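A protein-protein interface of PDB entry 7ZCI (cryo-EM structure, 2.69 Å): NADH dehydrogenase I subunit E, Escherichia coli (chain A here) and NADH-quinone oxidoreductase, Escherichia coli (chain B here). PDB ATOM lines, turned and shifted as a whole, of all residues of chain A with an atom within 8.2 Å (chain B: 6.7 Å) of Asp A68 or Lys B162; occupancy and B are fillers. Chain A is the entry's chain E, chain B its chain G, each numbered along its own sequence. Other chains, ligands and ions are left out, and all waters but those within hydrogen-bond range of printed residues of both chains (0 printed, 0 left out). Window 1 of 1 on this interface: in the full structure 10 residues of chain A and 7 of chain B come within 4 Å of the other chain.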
ATOM      1  N   ARG A  33      17.544  15.506   6.946  1.00  0.00           N
ATOM      2  CA  ARG A  33      18.713  15.271   7.795  1.00  0.00           C
ATOM      3  C   ARG A  33      18.511  15.830   9.196  1.00  0.00           C
ATOM      4  O   ARG A  33      19.046  15.288  10.167  1.00  0.00           O
ATOM      5  CB  ARG A  33      19.955  15.891   7.147  1.00  0.00           C
ATOM      6  CG  ARG A  33      21.253  15.755   7.924  1.00  0.00           C
ATOM      7  CD  ARG A  33      22.344  16.640   7.346  1.00  0.00           C
ATOM      8  NE  ARG A  33      22.722  16.192   6.014  1.00  0.00           N
ATOM      9  CZ  ARG A  33      23.623  15.252   5.768  1.00  0.00           C
ATOM     10  NH1 ARG A  33      24.313  14.685   6.742  1.00  0.00           N
ATOM     11  NH2 ARG A  33      23.833  14.870   4.513  1.00  0.00           N
ATOM     12  N   SER A  36      17.738  13.639  12.453  1.00  0.00           N
ATOM     13  CA  SER A  36      18.646  12.566  12.856  1.00  0.00           C
ATOM     14  C   SER A  36      18.747  12.445  14.369  1.00  0.00           C
ATOM     15  O   SER A  36      18.707  11.333  14.910  1.00  0.00           O
ATOM     16  CB  SER A  36      20.026  12.791  12.248  1.00  0.00           C
ATOM     17  OG  SER A  36      20.618  13.959  12.772  1.00  0.00           O
ATOM     18  N   LEU A  40      17.463   9.209  16.527  1.00  0.00           N
ATOM     19  CA  LEU A  40      18.311   8.504  17.477  1.00  0.00           C
ATOM     20  C   LEU A  40      17.680   8.488  18.861  1.00  0.00           C
ATOM     21  O   LEU A  40      17.703   7.462  19.546  1.00  0.00           O
ATOM     22  CB  LEU A  40      19.694   9.147  17.516  1.00  0.00           C
ATOM     23  CG  LEU A  40      20.565   8.925  16.281  1.00  0.00           C
ATOM     24  CD1 LEU A  40      21.656   9.967  16.205  1.00  0.00           C
ATOM     25  CD2 LEU A  40      21.158   7.540  16.278  1.00  0.00           C
ATOM     26  N   ILE A  55      21.972   2.524  13.374  1.00  0.00           N
ATOM     27  CA  ILE A  55      22.640   3.568  12.602  1.00  0.00           C
ATOM     28  C   ILE A  55      22.294   3.433  11.126  1.00  0.00           C
ATOM     29  O   ILE A  55      21.858   4.393  10.480  1.00  0.00           O
ATOM     30  CB  ILE A  55      24.161   3.506  12.830  1.00  0.00           C
ATOM     31  CG1 ILE A  55      24.495   3.741  14.305  1.00  0.00           C
ATOM     32  CG2 ILE A  55      24.876   4.514  11.949  1.00  0.00           C
ATOM     33  CD1 ILE A  55      24.162   5.125  14.801  1.00  0.00           C
ATOM     34  N   ILE A  58      18.356   4.039  10.589  1.00  0.00           N
ATOM     35  CA  ILE A  58      18.020   5.457  10.613  1.00  0.00           C
ATOM     36  C   ILE A  58      18.570   6.155   9.376  1.00  0.00           C
ATOM     37  O   ILE A  58      17.917   7.033   8.804  1.00  0.00           O
ATOM     38  CB  ILE A  58      18.544   6.090  11.916  1.00  0.00           C
ATOM     39  CG1 ILE A  58      17.677   5.673  13.098  1.00  0.00           C
ATOM     40  CG2 ILE A  58      18.587   7.601  11.837  1.00  0.00           C
ATOM     41  CD1 ILE A  58      18.331   5.934  14.420  1.00  0.00           C
ATOM     42  N   ALA A  59      19.765   5.756   8.929  1.00  0.00           N
ATOM     43  CA  ALA A  59      20.328   6.315   7.706  1.00  0.00           C
ATOM     44  C   ALA A  59      19.466   5.995   6.493  1.00  0.00           C
ATOM     45  O   ALA A  59      19.269   6.851   5.624  1.00  0.00           O
ATOM     46  CB  ALA A  59      21.743   5.784   7.501  1.00  0.00           C
ATOM     47  N   GLY A  63      17.705   8.975   4.536  1.00  0.00           N
ATOM     48  CA  GLY A  63      18.356   9.286   3.282  1.00  0.00           C
ATOM     49  C   GLY A  63      19.702   9.956   3.408  1.00  0.00           C
ATOM     50  O   GLY A  63      20.142  10.617   2.465  1.00  0.00           O
ATOM     51  N   ILE A  64      20.365   9.818   4.546  1.00  0.00           N
ATOM     52  CA  ILE A  64      21.704  10.359   4.758  1.00  0.00           C
ATOM     53  C   ILE A  64      22.637   9.172   4.957  1.00  0.00           C
ATOM     54  O   ILE A  64      22.171   8.053   5.225  1.00  0.00           O
ATOM     55  CB  ILE A  64      21.740  11.350   5.945  1.00  0.00           C
ATOM     56  CG1 ILE A  64      21.309  10.674   7.242  1.00  0.00           C
ATOM     57  CG2 ILE A  64      20.868  12.556   5.651  1.00  0.00           C
ATOM     58  CD1 ILE A  64      21.395  11.589   8.440  1.00  0.00           C
ATOM     59  N   PRO A  65      23.947   9.353   4.775  1.00  0.00           N
ATOM     60  CA  PRO A  65      24.876   8.239   4.991  1.00  0.00           C
ATOM     61  C   PRO A  65      24.890   7.755   6.432  1.00  0.00           C
ATOM     62  O   PRO A  65      24.597   8.493   7.374  1.00  0.00           O
ATOM     63  CB  PRO A  65      26.233   8.831   4.607  1.00  0.00           C
ATOM     64  CG  PRO A  65      25.914   9.892   3.654  1.00  0.00           C
ATOM     65  CD  PRO A  65      24.621  10.480   4.104  1.00  0.00           C
ATOM     66  N   ALA A  66      25.233   6.476   6.588  1.00  0.00           N
ATOM     67  CA  ALA A  66      25.388   5.910   7.923  1.00  0.00           C
ATOM     68  C   ALA A  66      26.566   6.524   8.668  1.00  0.00           C
ATOM     69  O   ALA A  66      26.562   6.549   9.902  1.00  0.00           O
ATOM     70  CB  ALA A  66      25.547   4.395   7.844  1.00  0.00           C
ATOM     71  N   SER A  67      27.570   7.028   7.945  1.00  0.00           N
ATOM     72  CA  SER A  67      28.679   7.715   8.597  1.00  0.00           C
ATOM     73  C   SER A  67      28.207   8.994   9.270  1.00  0.00           C
ATOM     74  O   SER A  67      28.665   9.327  10.368  1.00  0.00           O
ATOM     75  CB  SER A  67      29.789   8.020   7.594  1.00  0.00           C
ATOM     76  OG  SER A  67      29.352   8.914   6.591  1.00  0.00           O
ATOM     77  N   ASP A  68      27.284   9.717   8.633  1.00  0.00           N
ATOM     78  CA  ASP A  68      26.724  10.918   9.242  1.00  0.00           C
ATOM     79  C   ASP A  68      25.917  10.588  10.491  1.00  0.00           C
ATOM     80  O   ASP A  68      26.014  11.293  11.502  1.00  0.00           O
ATOM     81  CB  ASP A  68      25.861  11.662   8.227  1.00  0.00           C
ATOM     82  CG  ASP A  68      26.674  12.562   7.319  1.00  0.00           C
ATOM     83  OD1 ASP A  68      27.455  13.388   7.834  1.00  0.00           O
ATOM     84  OD2 ASP A  68      26.531  12.451   6.086  1.00  0.00           O
ATOM     85  N   VAL A  69      25.122   9.517  10.441  1.00  0.00           N
ATOM     86  CA  VAL A  69      24.332   9.109  11.601  1.00  0.00           C
ATOM     87  C   VAL A  69      25.240   8.689  12.746  1.00  0.00           C
ATOM     88  O   VAL A  69      25.002   9.046  13.904  1.00  0.00           O
ATOM     89  CB  VAL A  69      23.352   7.986  11.217  1.00  0.00           C
ATOM     90  CG1 VAL A  69      22.520   7.582  12.412  1.00  0.00           C
ATOM     91  CG2 VAL A  69      22.450   8.439  10.097  1.00  0.00           C
ATOM     92  N   GLU A  70      26.298   7.932  12.444  1.00  0.00           N
ATOM     93  CA  GLU A  70      27.226   7.514  13.487  1.00  0.00           C
ATOM     94  C   GLU A  70      27.985   8.703  14.057  1.00  0.00           C
ATOM     95  O   GLU A  70      28.240   8.757  15.265  1.00  0.00           O
ATOM     96  CB  GLU A  70      28.195   6.464  12.949  1.00  0.00           C
ATOM     97  CG  GLU A  70      29.080   5.852  14.019  1.00  0.00           C
ATOM     98  CD  GLU A  70      28.330   4.897  14.921  1.00  0.00           C
ATOM     99  OE1 GLU A  70      27.905   3.831  14.434  1.00  0.00           O
ATOM    100  OE2 GLU A  70      28.155   5.215  16.112  1.00  0.00           O
ATOM    101  N   GLY A  71      28.333   9.674  13.211  1.00  0.00           N
ATOM    102  CA  GLY A  71      28.993  10.872  13.698  1.00  0.00           C
ATOM    103  C   GLY A  71      28.118  11.684  14.627  1.00  0.00           C
ATOM    104  O   GLY A  71      28.583  12.186  15.650  1.00  0.00           O
ATOM    105  N   VAL A  72      26.834  11.808  14.291  1.00  0.00           N
ATOM    106  CA  VAL A  72      25.898  12.503  15.167  1.00  0.00           C
ATOM    107  C   VAL A  72      25.705  11.732  16.469  1.00  0.00           C
ATOM    108  O   VAL A  72      25.749  12.310  17.558  1.00  0.00           O
ATOM    109  CB  VAL A  72      24.563  12.740  14.439  1.00  0.00           C
ATOM    110  CG1 VAL A  72      23.492  13.165  15.408  1.00  0.00           C
ATOM    111  CG2 VAL A  72      24.741  13.794  13.376  1.00  0.00           C
ATOM    112  N   ALA A  73      25.524  10.413  16.379  1.00  0.00           N
ATOM    113  CA  ALA A  73      25.266   9.611  17.570  1.00  0.00           C
ATOM    114  C   ALA A  73      26.450   9.627  18.528  1.00  0.00           C
ATOM    115  O   ALA A  73      26.264   9.690  19.747  1.00  0.00           O
ATOM    116  CB  ALA A  73      24.916   8.180  17.176  1.00  0.00           C
ATOM    117  N   THR A  74      27.674   9.592  18.001  1.00  0.00           N
ATOM    118  CA  THR A  74      28.847   9.649  18.857  1.00  0.00           C
ATOM    119  C   THR A  74      29.246  11.066  19.236  1.00  0.00           C
ATOM    120  O   THR A  74      30.085  11.228  20.122  1.00  0.00           O
ATOM    121  CB  THR A  74      30.031   8.954  18.189  1.00  0.00           C
ATOM    122  OG1 THR A  74      30.322   9.597  16.945  1.00  0.00           O
ATOM    123  CG2 THR A  74      29.697   7.511  17.928  1.00  0.00           C
ATOM    124  N   PHE A  75      28.692  12.091  18.584  1.00  0.00           N
ATOM    125  CA  PHE A  75      28.966  13.457  19.015  1.00  0.00           C
ATOM    126  C   PHE A  75      28.216  13.802  20.292  1.00  0.00           C
ATOM    127  O   PHE A  75      28.775  14.430  21.194  1.00  0.00           O
ATOM    128  CB  PHE A  75      28.600  14.453  17.919  1.00  0.00           C
ATOM    129  CG  PHE A  75      28.979  15.868  18.246  1.00  0.00           C
ATOM    130  CD1 PHE A  75      30.260  16.315  18.017  1.00  0.00           C
ATOM    131  CD2 PHE A  75      28.057  16.747  18.793  1.00  0.00           C
ATOM    132  CE1 PHE A  75      30.616  17.601  18.315  1.00  0.00           C
ATOM    133  CE2 PHE A  75      28.413  18.036  19.103  1.00  0.00           C
ATOM    134  CZ  PHE A  75      29.693  18.464  18.860  1.00  0.00           C
ATOM    135  N   TYR A  76      26.947  13.430  20.377  1.00  0.00           N
ATOM    136  CA  TYR A  76      26.098  13.859  21.479  1.00  0.00           C
ATOM    137  C   TYR A  76      26.227  12.897  22.648  1.00  0.00           C
ATOM    138  O   TYR A  76      26.178  11.677  22.469  1.00  0.00           O
ATOM    139  CB  TYR A  76      24.647  13.980  21.019  1.00  0.00           C
ATOM    140  CG  TYR A  76      24.485  15.090  20.024  1.00  0.00           C
ATOM    141  CD1 TYR A  76      24.457  16.407  20.431  1.00  0.00           C
ATOM    142  CD2 TYR A  76      24.412  14.826  18.670  1.00  0.00           C
ATOM    143  CE1 TYR A  76      24.339  17.422  19.521  1.00  0.00           C
ATOM    144  CE2 TYR A  76      24.301  15.833  17.755  1.00  0.00           C
ATOM    145  CZ  TYR A  76      24.265  17.128  18.186  1.00  0.00           C
ATOM    146  OH  TYR A  76      24.149  18.139  17.274  1.00  0.00           O
ATOM    147  N   CYS B 157      40.670  14.846   5.492  1.00  0.00           N
ATOM    148  CA  CYS B 157      40.196  13.583   4.941  1.00  0.00           C
ATOM    149  C   CYS B 157      38.698  13.603   4.712  1.00  0.00           C
ATOM    150  O   CYS B 157      38.223  13.206   3.647  1.00  0.00           O
ATOM    151  CB  CYS B 157      40.555  12.432   5.873  1.00  0.00           C
ATOM    152  SG  CYS B 157      39.957  12.665   7.538  1.00  0.00           S
ATOM    153  N   VAL B 158      37.934  14.030   5.714  1.00  0.00           N
ATOM    154  CA  VAL B 158      36.488  14.025   5.570  1.00  0.00           C
ATOM    155  C   VAL B 158      36.052  15.077   4.566  1.00  0.00           C
ATOM    156  O   VAL B 158      35.143  14.840   3.771  1.00  0.00           O
ATOM    157  CB  VAL B 158      35.790  14.191   6.934  1.00  0.00           C
ATOM    158  CG1 VAL B 158      35.931  12.923   7.725  1.00  0.00           C
ATOM    159  CG2 VAL B 158      36.329  15.386   7.719  1.00  0.00           C
ATOM    160  N   ARG B 159      36.714  16.235   4.556  1.00  0.00           N
ATOM    161  CA  ARG B 159      36.335  17.285   3.620  1.00  0.00           C
ATOM    162  C   ARG B 159      36.595  16.858   2.184  1.00  0.00           C
ATOM    163  O   ARG B 159      35.701  16.983   1.345  1.00  0.00           O
ATOM    164  CB  ARG B 159      37.057  18.584   3.955  1.00  0.00           C
ATOM    165  CG  ARG B 159      36.512  19.213   5.218  1.00  0.00           C
ATOM    166  CD  ARG B 159      36.855  20.664   5.353  1.00  0.00           C
ATOM    167  NE  ARG B 159      38.243  20.963   5.040  1.00  0.00           N
ATOM    168  CZ  ARG B 159      38.630  21.765   4.060  1.00  0.00           C
ATOM    169  NH1 ARG B 159      37.760  22.314   3.233  1.00  0.00           N
ATOM    170  NH2 ARG B 159      39.921  22.025   3.908  1.00  0.00           N
ATOM    171  N   TYR B 160      37.746  16.235   1.917  1.00  0.00           N
ATOM    172  CA  TYR B 160      37.991  15.655   0.600  1.00  0.00           C
ATOM    173  C   TYR B 160      36.975  14.563   0.285  1.00  0.00           C
ATOM    174  O   TYR B 160      36.164  14.705  -0.635  1.00  0.00           O
ATOM    175  CB  TYR B 160      39.415  15.093   0.508  1.00  0.00           C
ATOM    176  CG  TYR B 160      39.572  14.133  -0.647  1.00  0.00           C
ATOM    177  CD1 TYR B 160      39.556  14.594  -1.955  1.00  0.00           C
ATOM    178  CD2 TYR B 160      39.683  12.764  -0.439  1.00  0.00           C
ATOM    179  CE1 TYR B 160      39.660  13.728  -3.010  1.00  0.00           C
ATOM    180  CE2 TYR B 160      39.781  11.893  -1.491  1.00  0.00           C
ATOM    181  CZ  TYR B 160      39.779  12.386  -2.772  1.00  0.00           C
ATOM    182  OH  TYR B 160      39.886  11.530  -3.828  1.00  0.00           O
ATOM    183  N   TYR B 161      36.968  13.498   1.089  1.00  0.00           N
ATOM    184  CA  TYR B 161      36.228  12.278   0.784  1.00  0.00           C
ATOM    185  C   TYR B 161      34.728  12.508   0.702  1.00  0.00           C
ATOM    186  O   TYR B 161      34.048  11.829  -0.068  1.00  0.00           O
ATOM    187  CB  TYR B 161      36.543  11.230   1.849  1.00  0.00           C
ATOM    188  CG  TYR B 161      36.194   9.801   1.508  1.00  0.00           C
ATOM    189  CD1 TYR B 161      34.914   9.316   1.712  1.00  0.00           C
ATOM    190  CD2 TYR B 161      37.149   8.934   1.011  1.00  0.00           C
ATOM    191  CE1 TYR B 161      34.593   8.020   1.424  1.00  0.00           C
ATOM    192  CE2 TYR B 161      36.832   7.631   0.722  1.00  0.00           C
ATOM    193  CZ  TYR B 161      35.551   7.184   0.932  1.00  0.00           C
ATOM    194  OH  TYR B 161      35.207   5.895   0.649  1.00  0.00           O
ATOM    195  N   LYS B 162      34.197  13.472   1.446  1.00  0.00           N
ATOM    196  CA  LYS B 162      32.765  13.691   1.519  1.00  0.00           C
ATOM    197  C   LYS B 162      32.317  14.933   0.766  1.00  0.00           C
ATOM    198  O   LYS B 162      31.369  14.860  -0.012  1.00  0.00           O
ATOM    199  CB  LYS B 162      32.350  13.781   2.992  1.00  0.00           C
ATOM    200  CG  LYS B 162      30.883  14.020   3.225  1.00  0.00           C
ATOM    201  CD  LYS B 162      30.493  13.666   4.647  1.00  0.00           C
ATOM    202  CE  LYS B 162      30.633  12.179   4.894  1.00  0.00           C
ATOM    203  NZ  LYS B 162      30.318  11.805   6.298  1.00  0.00           N
ATOM    204  N   ASP B 163      32.953  16.083   0.988  1.00  0.00           N
ATOM    205  CA  ASP B 163      32.504  17.292   0.327  1.00  0.00           C
ATOM    206  C   ASP B 163      33.098  17.442  -1.064  1.00  0.00           C
ATOM    207  O   ASP B 163      32.568  18.216  -1.861  1.00  0.00           O
ATOM    208  CB  ASP B 163      32.853  18.513   1.177  1.00  0.00           C
ATOM    209  CG  ASP B 163      32.389  18.380   2.609  1.00  0.00           C
ATOM    210  OD1 ASP B 163      31.337  17.749   2.839  1.00  0.00           O
ATOM    211  OD2 ASP B 163      33.064  18.915   3.510  1.00  0.00           O
ATOM    212  N   TYR B 164      34.200  16.756  -1.376  1.00  0.00           N
ATOM    213  CA  TYR B 164      34.788  16.826  -2.708  1.00  0.00           C
ATOM    214  C   TYR B 164      34.465  15.594  -3.546  1.00  0.00           C
ATOM    215  O   TYR B 164      33.938  15.720  -4.653  1.00  0.00           O
ATOM    216  CB  TYR B 164      36.308  17.033  -2.617  1.00  0.00           C
ATOM    217  CG  TYR B 164      36.937  17.484  -3.916  1.00  0.00           C
ATOM    218  CD1 TYR B 164      37.343  16.562  -4.869  1.00  0.00           C
ATOM    219  CD2 TYR B 164      37.109  18.825  -4.198  1.00  0.00           C
ATOM    220  CE1 TYR B 164      37.890  16.961  -6.056  1.00  0.00           C
ATOM    221  CE2 TYR B 164      37.677  19.235  -5.381  1.00  0.00           C
ATOM    222  CZ  TYR B 164      38.062  18.299  -6.307  1.00  0.00           C
ATOM    223  OH  TYR B 164      38.625  18.702  -7.489  1.00  0.00           O
ATOM    224  N   ALA B 165      34.795  14.406  -3.052  1.00  0.00           N
ATOM    225  CA  ALA B 165      34.627  13.176  -3.814  1.00  0.00           C
ATOM    226  C   ALA B 165      33.265  12.536  -3.616  1.00  0.00           C
ATOM    227  O   ALA B 165      32.979  11.528  -4.265  1.00  0.00           O
ATOM    228  CB  ALA B 165      35.717  12.169  -3.447  1.00  0.00           C
ATOM    229  N   ASP B 166      32.437  13.094  -2.727  1.00  0.00           N
ATOM    230  CA  ASP B 166      31.080  12.620  -2.443  1.00  0.00           C
ATOM    231  C   ASP B 166      31.051  11.159  -2.008  1.00  0.00           C
ATOM    232  O   ASP B 166      30.114  10.426  -2.322  1.00  0.00           O
ATOM    233  CB  ASP B 166      30.140  12.841  -3.632  1.00  0.00           C
ATOM    234  CG  ASP B 166      30.088  14.288  -4.074  1.00  0.00           C
ATOM    235  OD1 ASP B 166      30.273  15.180  -3.224  1.00  0.00           O
ATOM    236  OD2 ASP B 166      29.861  14.539  -5.272  1.00  0.00           O
ATOM    237  N   GLY B 167      32.076  10.719  -1.291  1.00  0.00           N
ATOM    238  CA  GLY B 167      32.023   9.426  -0.652  1.00  0.00           C
ATOM    239  C   GLY B 167      31.167   9.467   0.597  1.00  0.00           C
ATOM    240  O   GLY B 167      31.037  10.492   1.263  1.00  0.00           O
ATOM    241  N   THR B 168      30.578   8.322   0.923  1.00  0.00           N
ATOM    242  CA  THR B 168      29.601   8.249   1.994  1.00  0.00           C
ATOM    243  C   THR B 168      30.072   7.480   3.216  1.00  0.00           C
ATOM    244  O   THR B 168      29.454   7.609   4.275  1.00  0.00           O
ATOM    245  CB  THR B 168      28.303   7.606   1.487  1.00  0.00           C
ATOM    246  OG1 THR B 168      28.597   6.343   0.879  1.00  0.00           O
ATOM    247  CG2 THR B 168      27.624   8.503   0.473  1.00  0.00           C
ATOM    248  N   ASP B 169      31.138   6.691   3.107  1.00  0.00           N
ATOM    249  CA  ASP B 169      31.504   5.750   4.155  1.00  0.00           C
ATOM    250  C   ASP B 169      32.720   6.189   4.960  1.00  0.00           C
ATOM    251  O   ASP B 169      33.349   5.356   5.612  1.00  0.00           O
ATOM    252  CB  ASP B 169      31.741   4.365   3.559  1.00  0.00           C
ATOM    253  CG  ASP B 169      32.765   4.375   2.453  1.00  0.00           C
ATOM    254  OD1 ASP B 169      32.837   5.379   1.724  1.00  0.00           O
ATOM    255  OD2 ASP B 169      33.485   3.375   2.297  1.00  0.00           O
ATOM    256  N   LEU B 170      33.072   7.465   4.928  1.00  0.00           N
ATOM    257  CA  LEU B 170      34.088   8.002   5.816  1.00  0.00           C
ATOM    258  C   LEU B 170      33.526   9.216   6.529  1.00  0.00           C
ATOM    259  O   LEU B 170      32.823  10.027   5.928  1.00  0.00           O
ATOM    260  CB  LEU B 170      35.364   8.381   5.065  1.00  0.00           C
ATOM    261  CG  LEU B 170      36.601   8.659   5.920  1.00  0.00           C
ATOM    262  CD1 LEU B 170      37.438   7.410   6.069  1.00  0.00           C
ATOM    263  CD2 LEU B 170      37.421   9.802   5.352  1.00  0.00           C
ATOM    264  N   GLY B 171      33.838   9.338   7.810  1.00  0.00           N
ATOM    265  CA  GLY B 171      33.344  10.468   8.565  1.00  0.00           C
ATOM    266  C   GLY B 171      34.127  10.661   9.840  1.00  0.00           C
ATOM    267  O   GLY B 171      35.023   9.883  10.182  1.00  0.00           O
ATOM    268  N   VAL B 172      33.764  11.725  10.543  1.00  0.00           N
ATOM    269  CA  VAL B 172      34.313  12.051  11.848  1.00  0.00           C
ATOM    270  C   VAL B 172      33.290  11.651  12.905  1.00  0.00           C
ATOM    271  O   VAL B 172      32.084  11.865  12.739  1.00  0.00           O
ATOM    272  CB  VAL B 172      34.724  13.537  11.936  1.00  0.00           C
ATOM    273  CG1 VAL B 172      33.549  14.468  11.786  1.00  0.00           C
ATOM    274  CG2 VAL B 172      35.437  13.816  13.239  1.00  0.00           C
ATOM    275  N   TYR B 173      33.770  10.994  13.951  1.00  0.00           N
ATOM    276  CA  TYR B 173      32.965  10.519  15.059  1.00  0.00           C
ATOM    277  C   TYR B 173      33.535  11.048  16.360  1.00  0.00           C
ATOM    278  O   TYR B 173      34.664  11.533  16.418  1.00  0.00           O
ATOM    279  CB  TYR B 173      32.911   8.995  15.095  1.00  0.00           C
ATOM    280  CG  TYR B 173      32.808   8.414  13.725  1.00  0.00           C
ATOM    281  CD1 TYR B 173      31.619   8.484  13.025  1.00  0.00           C
ATOM    282  CD2 TYR B 173      33.899   7.822  13.117  1.00  0.00           C
ATOM    283  CE1 TYR B 173      31.512   7.975  11.769  1.00  0.00           C
ATOM    284  CE2 TYR B 173      33.801   7.310  11.859  1.00  0.00           C
ATOM    285  CZ  TYR B 173      32.604   7.395  11.188  1.00  0.00           C
ATOM    286  OH  TYR B 173      32.491   6.892   9.925  1.00  0.00           O
ATOM    287  N   LYS B 398      28.644  20.748  -8.258  1.00  0.00           N
ATOM    288  CA  LYS B 398      28.707  21.704  -7.142  1.00  0.00           C
ATOM    289  C   LYS B 398      28.878  23.159  -7.593  1.00  0.00           C
ATOM    290  O   LYS B 398      28.795  24.087  -6.759  1.00  0.00           O
ATOM    291  CB  LYS B 398      29.837  21.306  -6.199  1.00  0.00           C
ATOM    292  CG  LYS B 398      29.675  19.910  -5.640  1.00  0.00           C
ATOM    293  CD  LYS B 398      30.589  19.672  -4.464  1.00  0.00           C
ATOM    294  CE  LYS B 398      31.825  18.920  -4.885  1.00  0.00           C
ATOM    295  NZ  LYS B 398      31.547  17.470  -5.050  1.00  0.00           N
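The side-chain hydroxyl of Ser A67 lies within hydrogen-bond range of the side-chain amino group of Lys B162, at 3.1 Å.
OG of Ser A67 is in hydrogen-bond range of O of Thr B168 (2.7 Å).
NZ of Lys B162 is in salt-bridge range of OD1 of Asp A68, 3.6 Å away.
OD2 of Asp A68 lies within salt-bridge range of NH1 of Arg A33 (3.2 Å).
The backbone carbonyl oxygen of Glu A70 lies within hydrogen-bond range of the side-chain hydroxyl of Thr A74 (2.8 Å).
OG1 of Thr A74 sits at hydrogen-bond distance from O of Gly A71 (3.4 Å).
The side-chain amino group (NZ) of Lys B162 sits at hydrogen-bond distance from the backbone carbonyl oxygen (O) of Leu B170, 3.1 Å away.
O of Thr B168 touches CB of Pro A65 (3.5 Å).
OG of Ser A67 touches O of Leu B170, at 3.7 Å.
Ser A67 touches Tyr B173.
Glu A70 touches Tyr B173.
Gly A71 touches Val B172.
Tyr B173 touches Gly A71 (CD1 to N, 3.5 Å).
Tyr B173 touches Thr A74.
Asp A68 touches one residue of chain B.
Of the printed residues of chain B, Gly A71 touches Val B172 (3.4 Å) and Tyr B173 (3.5 Å).
Of the printed residues of chain B, Thr A74 touches Tyr B173 (3.2 Å).
Printed residues of chain A within 4 Å of Lys B162: Ser A67 (3.1 Å) and Asp A68 (3.6 Å).
Printed residues of chain A within 4 Å of Tyr B173: Ser A67, Glu A70, Gly A71 and Thr A74.
The nearest residue of chain A that does not touch Lys B162 is Pro A65 (5.3 Å).
The nearest printed residue of chain B that does not touch Gly A71 is Gly B171 (6.4 Å).
Of the 20 printed residues of chain A, 6 touch a printed residue of chain B.
Among the printed residues, 10 pairs touch across the chains.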
